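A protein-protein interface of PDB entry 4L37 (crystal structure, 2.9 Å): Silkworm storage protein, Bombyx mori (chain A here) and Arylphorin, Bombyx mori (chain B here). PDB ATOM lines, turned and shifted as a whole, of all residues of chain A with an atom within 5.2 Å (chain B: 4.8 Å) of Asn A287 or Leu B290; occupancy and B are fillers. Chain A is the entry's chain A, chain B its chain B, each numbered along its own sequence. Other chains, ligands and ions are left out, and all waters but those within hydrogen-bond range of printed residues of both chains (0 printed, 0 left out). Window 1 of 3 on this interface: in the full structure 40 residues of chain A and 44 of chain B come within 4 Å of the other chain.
The side-chain amide oxygen of Gln B161 sits at hydrogen-bond distance from the side-chain amide nitrogen of Asn A287 (2.6 Å). The backbone carbonyl oxygen (O) of Ser A288 sits at hydrogen-bond distance from the side-chain amide nitrogen (NE2) of Gln B161, 3.2 Å away. The side-chain amide nitrogen of Gln B161 lies within hydrogen-bond range of the backbone carbonyl oxygen of Phe A289 (3.4 Å). The side-chain sulfur (SD) of Met B157 lies close to the backbone nitrogen (N) of Pro A292 (3.5 Å).
The side-chain hydroxyl (OG) of Ser A288 is in hydrogen-bond range of the backbone NH (N) of Tyr A291 (3.2 Å). N of Met B157 lies within hydrogen-bond range of O of Leu B288, at 2.8 Å.
ND2 of Asn A287 touches CE of Met B157, 3.3 Å away. Asn A287 touches Leu B290. Met B157 touches Ser A288. O of Phe A289 touches CE of Met B157, at 3.6 Å. Tyr A291 touches Met B157 (C to SD, 3.5 Å). Pro A292 touches Leu B288 (CD to CD2, 3.6 Å).
Asn A287 touches just these residues of chain B: Met B157, Gln B161 and Leu B290. Printed residues of chain B within 4 Å of Phe A289: Met B157 (3.6 Å) and Gln B161 (3.4 Å). Printed residues of chain B within 4 Å of Tyr A291: Met B157 (3.5 Å). Of the printed residues of chain A, Met B157 touches Asn A287, Ser A288, Phe A289, Tyr A291 and Pro A292. Of chain A, only Asn A287 (3.4 Å) comes within 4 Å of Leu B290. Phe B296 touches none of the printed residues of chain A. The nearest printed residue of chain B that does not touch Asn A287 is Pro B295 (6.3 Å). The nearest printed residue of chain B that does not touch Phe A289 is Leu B160 (7.5 Å).
Of the 11 printed residues of chain B, 4 touch a printed residue of chain A. Hydrophobic or aromatic side chains of chain B within 4 Å of the printed part of chain A: Met B157, Leu B288 and Leu B290. Of the 9 printed residues of chain A, 5 touch a printed residue of chain B. Printed residues of chain A that touch a printed residue of chain B: Asn A287, Ser A288, Phe A289, Tyr A291 and Pro A292. Among the printed residues, no Asp or Glu carboxylate lies within 4 Å of a Lys or Arg side-chain nitrogen of the other chain.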
ATOM      1  N   MET A 154       7.562   1.507  11.384  1.00  0.00           N
ATOM      2  CA  MET A 154       8.631   2.056  10.570  1.00  0.00           C
ATOM      3  C   MET A 154       9.845   2.652  11.297  1.00  0.00           C
ATOM      4  O   MET A 154      10.923   2.752  10.716  1.00  0.00           O
ATOM      5  CB  MET A 154       8.095   2.937   9.464  1.00  0.00           C
ATOM      6  CG  MET A 154       7.891   4.370   9.815  1.00  0.00           C
ATOM      7  SD  MET A 154       8.015   5.364   8.306  1.00  0.00           S
ATOM      8  CE  MET A 154       6.829   4.570   7.217  1.00  0.00           C
ATOM      9  N   PRO A 285       1.723   2.774  10.108  1.00  0.00           N
ATOM     10  CA  PRO A 285       3.183   3.063  10.165  1.00  0.00           C
ATOM     11  C   PRO A 285       3.981   2.231   9.152  1.00  0.00           C
ATOM     12  O   PRO A 285       4.905   1.503   9.542  1.00  0.00           O
ATOM     13  CB  PRO A 285       3.565   2.605  11.577  1.00  0.00           C
ATOM     14  CG  PRO A 285       2.667   1.425  11.795  1.00  0.00           C
ATOM     15  CD  PRO A 285       1.340   1.811  11.167  1.00  0.00           C
ATOM     16  N   PHE A 286       3.611   2.331   7.881  1.00  0.00           N
ATOM     17  CA  PHE A 286       4.190   1.518   6.852  1.00  0.00           C
ATOM     18  C   PHE A 286       4.381   2.365   5.623  1.00  0.00           C
ATOM     19  O   PHE A 286       3.703   3.392   5.449  1.00  0.00           O
ATOM     20  CB  PHE A 286       3.232   0.369   6.505  1.00  0.00           C
ATOM     21  CG  PHE A 286       3.043  -0.637   7.620  1.00  0.00           C
ATOM     22  CD1 PHE A 286       4.099  -1.453   8.044  1.00  0.00           C
ATOM     23  CD2 PHE A 286       1.815  -0.767   8.250  1.00  0.00           C
ATOM     24  CE1 PHE A 286       3.924  -2.363   9.071  1.00  0.00           C
ATOM     25  CE2 PHE A 286       1.640  -1.683   9.276  1.00  0.00           C
ATOM     26  CZ  PHE A 286       2.699  -2.468   9.690  1.00  0.00           C
ATOM     27  N   ASN A 287       5.296   1.932   4.763  1.00  0.00           N
ATOM     28  CA  ASN A 287       5.364   2.460   3.414  1.00  0.00           C
ATOM     29  C   ASN A 287       5.703   1.387   2.371  1.00  0.00           C
ATOM     30  O   ASN A 287       6.443   0.486   2.628  1.00  0.00           O
ATOM     31  CB  ASN A 287       6.329   3.649   3.359  1.00  0.00           C
ATOM     32  CG  ASN A 287       7.776   3.227   3.416  1.00  0.00           C
ATOM     33  OD1 ASN A 287       8.397   3.288   4.478  1.00  0.00           O
ATOM     34  ND2 ASN A 287       8.325   2.783   2.278  1.00  0.00           N
ATOM     35  N   SER A 288       5.136   1.495   1.187  1.00  0.00           N
ATOM     36  CA  SER A 288       5.487   0.613   0.089  1.00  0.00           C
ATOM     37  C   SER A 288       6.676   1.192  -0.705  1.00  0.00           C
ATOM     38  O   SER A 288       7.303   2.159  -0.271  1.00  0.00           O
ATOM     39  CB  SER A 288       4.265   0.425  -0.820  1.00  0.00           C
ATOM     40  OG  SER A 288       4.307   1.278  -1.970  1.00  0.00           O
ATOM     41  N   PHE A 289       6.968   0.584  -1.864  1.00  0.00           N
ATOM     42  CA  PHE A 289       7.998   1.026  -2.795  1.00  0.00           C
ATOM     43  C   PHE A 289       7.734   2.445  -3.266  1.00  0.00           C
ATOM     44  O   PHE A 289       8.602   3.271  -3.175  1.00  0.00           O
ATOM     45  CB  PHE A 289       8.041   0.072  -3.982  1.00  0.00           C
ATOM     46  CG  PHE A 289       9.260   0.227  -4.870  1.00  0.00           C
ATOM     47  CD1 PHE A 289      10.531  -0.194  -4.439  1.00  0.00           C
ATOM     48  CD2 PHE A 289       9.134   0.746  -6.179  1.00  0.00           C
ATOM     49  CE1 PHE A 289      11.639  -0.062  -5.272  1.00  0.00           C
ATOM     50  CE2 PHE A 289      10.246   0.884  -7.019  1.00  0.00           C
ATOM     51  CZ  PHE A 289      11.498   0.476  -6.566  1.00  0.00           C
ATOM     52  N   TYR A 291       4.741   4.417  -2.236  1.00  0.00           N
ATOM     53  CA  TYR A 291       3.827   5.227  -1.395  1.00  0.00           C
ATOM     54  C   TYR A 291       3.973   4.970   0.082  1.00  0.00           C
ATOM     55  O   TYR A 291       4.213   3.842   0.487  1.00  0.00           O
ATOM     56  CB  TYR A 291       2.361   4.954  -1.703  1.00  0.00           C
ATOM     57  CG  TYR A 291       1.996   4.899  -3.161  1.00  0.00           C
ATOM     58  CD1 TYR A 291       1.801   6.066  -3.915  1.00  0.00           C
ATOM     59  CD2 TYR A 291       1.805   3.666  -3.787  1.00  0.00           C
ATOM     60  CE1 TYR A 291       1.439   5.991  -5.255  1.00  0.00           C
ATOM     61  CE2 TYR A 291       1.472   3.588  -5.119  1.00  0.00           C
ATOM     62  CZ  TYR A 291       1.287   4.746  -5.842  1.00  0.00           C
ATOM     63  OH  TYR A 291       0.958   4.628  -7.164  1.00  0.00           O
ATOM     64  N   PRO A 292       3.816   6.030   0.897  1.00  0.00           N
ATOM     65  CA  PRO A 292       3.527   5.775   2.285  1.00  0.00           C
ATOM     66  C   PRO A 292       2.116   5.281   2.280  1.00  0.00           C
ATOM     67  O   PRO A 292       1.347   5.674   1.407  1.00  0.00           O
ATOM     68  CB  PRO A 292       3.561   7.161   2.919  1.00  0.00           C
ATOM     69  CG  PRO A 292       4.293   8.022   1.954  1.00  0.00           C
ATOM     70  CD  PRO A 292       3.948   7.468   0.615  1.00  0.00           C
ATOM     71  N   PHE A 293       1.785   4.423   3.229  1.00  0.00           N
ATOM     72  CA  PHE A 293       0.434   3.925   3.410  1.00  0.00           C
ATOM     73  C   PHE A 293      -0.617   5.019   3.573  1.00  0.00           C
ATOM     74  O   PHE A 293      -0.339   6.100   4.032  1.00  0.00           O
ATOM     75  CB  PHE A 293       0.427   3.024   4.646  1.00  0.00           C
ATOM     76  CG  PHE A 293       0.690   1.567   4.342  1.00  0.00           C
ATOM     77  CD1 PHE A 293      -0.107   0.565   4.900  1.00  0.00           C
ATOM     78  CD2 PHE A 293       1.721   1.188   3.479  1.00  0.00           C
ATOM     79  CE1 PHE A 293       0.138  -0.777   4.622  1.00  0.00           C
ATOM     80  CE2 PHE A 293       1.961  -0.153   3.205  1.00  0.00           C
ATOM     81  CZ  PHE A 293       1.173  -1.134   3.780  1.00  0.00           C
ATOM     82  N   MET B 157       9.809   9.584  -1.678  1.00  0.00           N
ATOM     83  CA  MET B 157      10.345   8.465  -0.909  1.00  0.00           C
ATOM     84  C   MET B 157      10.736   7.293  -1.780  1.00  0.00           C
ATOM     85  O   MET B 157      11.665   6.553  -1.423  1.00  0.00           O
ATOM     86  CB  MET B 157       9.376   7.997   0.168  1.00  0.00           C
ATOM     87  CG  MET B 157       7.980   7.741  -0.372  1.00  0.00           C
ATOM     88  SD  MET B 157       7.244   6.224   0.255  1.00  0.00           S
ATOM     89  CE  MET B 157       8.627   5.117  -0.037  1.00  0.00           C
ATOM     90  N   LEU B 160      14.370   8.034  -2.443  1.00  0.00           N
ATOM     91  CA  LEU B 160      15.128   7.901  -1.197  1.00  0.00           C
ATOM     92  C   LEU B 160      15.368   6.431  -0.845  1.00  0.00           C
ATOM     93  O   LEU B 160      16.485   6.044  -0.504  1.00  0.00           O
ATOM     94  CB  LEU B 160      14.434   8.586  -0.036  1.00  0.00           C
ATOM     95  CG  LEU B 160      15.302   8.631   1.222  1.00  0.00           C
ATOM     96  CD1 LEU B 160      16.433   9.610   0.995  1.00  0.00           C
ATOM     97  CD2 LEU B 160      14.506   9.060   2.430  1.00  0.00           C
ATOM     98  N   GLN B 161      14.323   5.613  -0.966  1.00  0.00           N
ATOM     99  CA  GLN B 161      14.431   4.204  -0.649  1.00  0.00           C
ATOM    100  C   GLN B 161      15.377   3.489  -1.566  1.00  0.00           C
ATOM    101  O   GLN B 161      16.115   2.603  -1.128  1.00  0.00           O
ATOM    102  CB  GLN B 161      13.080   3.523  -0.679  1.00  0.00           C
ATOM    103  CG  GLN B 161      12.573   3.210   0.715  1.00  0.00           C
ATOM    104  CD  GLN B 161      11.181   2.601   0.699  1.00  0.00           C
ATOM    105  OE1 GLN B 161      10.715   2.062   1.714  1.00  0.00           O
ATOM    106  NE2 GLN B 161      10.504   2.678  -0.457  1.00  0.00           N
ATOM    107  N   LEU B 288       4.627  12.401  -0.570  1.00  0.00           N
ATOM    108  CA  LEU B 288       5.294  11.132  -0.700  1.00  0.00           C
ATOM    109  C   LEU B 288       6.694  11.276  -0.183  1.00  0.00           C
ATOM    110  O   LEU B 288       7.626  11.162  -0.936  1.00  0.00           O
ATOM    111  CB  LEU B 288       5.327  10.692  -2.152  1.00  0.00           C
ATOM    112  CG  LEU B 288       4.002  10.540  -2.916  1.00  0.00           C
ATOM    113  CD1 LEU B 288       4.239  10.254  -4.429  1.00  0.00           C
ATOM    114  CD2 LEU B 288       3.136   9.500  -2.208  1.00  0.00           C
ATOM    115  N   MET B 289       6.811  11.500   1.124  1.00  0.00           N
ATOM    116  CA  MET B 289       8.071  11.800   1.794  1.00  0.00           C
ATOM    117  C   MET B 289       7.976  11.263   3.199  1.00  0.00           C
ATOM    118  O   MET B 289       6.851  11.128   3.737  1.00  0.00           O
ATOM    119  CB  MET B 289       8.183  13.283   1.917  1.00  0.00           C
ATOM    120  CG  MET B 289       9.504  13.850   1.506  1.00  0.00           C
ATOM    121  SD  MET B 289       9.197  15.576   1.144  1.00  0.00           S
ATOM    122  CE  MET B 289       7.652  15.506   0.191  1.00  0.00           C
ATOM    123  N   LEU B 290       9.129  10.960   3.807  1.00  0.00           N
ATOM    124  CA  LEU B 290       9.114  10.500   5.220  1.00  0.00           C
ATOM    125  C   LEU B 290      10.319  10.909   6.100  1.00  0.00           C
ATOM    126  O   LEU B 290      11.281  11.549   5.624  1.00  0.00           O
ATOM    127  CB  LEU B 290       8.818   8.976   5.321  1.00  0.00           C
ATOM    128  CG  LEU B 290       9.408   8.040   4.240  1.00  0.00           C
ATOM    129  CD1 LEU B 290      10.943   7.890   4.294  1.00  0.00           C
ATOM    130  CD2 LEU B 290       8.689   6.688   4.261  1.00  0.00           C
ATOM    131  N   THR B 291      10.225  10.540   7.383  1.00  0.00           N
ATOM    132  CA  THR B 291      11.274  10.775   8.382  1.00  0.00           C
ATOM    133  C   THR B 291      11.555   9.527   9.235  1.00  0.00           C
ATOM    134  O   THR B 291      10.663   8.712   9.508  1.00  0.00           O
ATOM    135  CB  THR B 291      10.902  11.940   9.334  1.00  0.00           C
ATOM    136  OG1 THR B 291       9.777  11.566  10.153  1.00  0.00           O
ATOM    137  CG2 THR B 291      10.610  13.253   8.536  1.00  0.00           C
ATOM    138  N   LYS B 292      12.797   9.405   9.677  1.00  0.00           N
ATOM    139  CA  LYS B 292      13.220   8.278  10.510  1.00  0.00           C
ATOM    140  C   LYS B 292      12.190   7.760  11.540  1.00  0.00           C
ATOM    141  O   LYS B 292      12.435   6.785  12.249  1.00  0.00           O
ATOM    142  CB  LYS B 292      14.511   8.633  11.271  1.00  0.00           C
ATOM    143  CG  LYS B 292      15.571   9.435  10.522  1.00  0.00           C
ATOM    144  CD  LYS B 292      16.766   9.680  11.446  1.00  0.00           C
ATOM    145  CE  LYS B 292      17.850  10.541  10.807  1.00  0.00           C
ATOM    146  NZ  LYS B 292      17.483  11.979  10.682  1.00  0.00           N
ATOM    147  N   THR B 294       8.437   8.647  11.104  1.00  0.00           N
ATOM    148  CA  THR B 294       7.067   8.782  10.627  1.00  0.00           C
ATOM    149  C   THR B 294       6.997   9.293   9.218  1.00  0.00           C
ATOM    150  O   THR B 294       7.939   9.928   8.726  1.00  0.00           O
ATOM    151  CB  THR B 294       6.217   9.746  11.502  1.00  0.00           C
ATOM    152  OG1 THR B 294       7.085  10.502  12.362  1.00  0.00           O
ATOM    153  CG2 THR B 294       5.156   8.971  12.329  1.00  0.00           C
ATOM    154  N   PRO B 295       5.859   9.008   8.570  1.00  0.00           N
ATOM    155  CA  PRO B 295       5.548   9.618   7.289  1.00  0.00           C
ATOM    156  C   PRO B 295       4.978  11.019   7.476  1.00  0.00           C
ATOM    157  O   PRO B 295       4.371  11.301   8.514  1.00  0.00           O
ATOM    158  CB  PRO B 295       4.479   8.686   6.700  1.00  0.00           C
ATOM    159  CG  PRO B 295       3.947   7.855   7.833  1.00  0.00           C
ATOM    160  CD  PRO B 295       4.822   8.059   9.034  1.00  0.00           C
ATOM    161  N   PHE B 296       5.160  11.885   6.492  1.00  0.00           N
ATOM    162  CA  PHE B 296       4.430  13.133   6.457  1.00  0.00           C
ATOM    163  C   PHE B 296       2.927  12.859   6.444  1.00  0.00           C
ATOM    164  O   PHE B 296       2.473  11.868   5.847  1.00  0.00           O
ATOM    165  CB  PHE B 296       4.794  13.909   5.193  1.00  0.00           C
ATOM    166  CG  PHE B 296       6.114  14.629   5.265  1.00  0.00           C
ATOM    167  CD1 PHE B 296       7.267  13.988   5.756  1.00  0.00           C
ATOM    168  CD2 PHE B 296       6.216  15.927   4.835  1.00  0.00           C
ATOM    169  CE1 PHE B 296       8.490  14.643   5.849  1.00  0.00           C
ATOM    170  CE2 PHE B 296       7.437  16.581   4.902  1.00  0.00           C
ATOM    171  CZ  PHE B 296       8.582  15.943   5.410  1.00  0.00           C
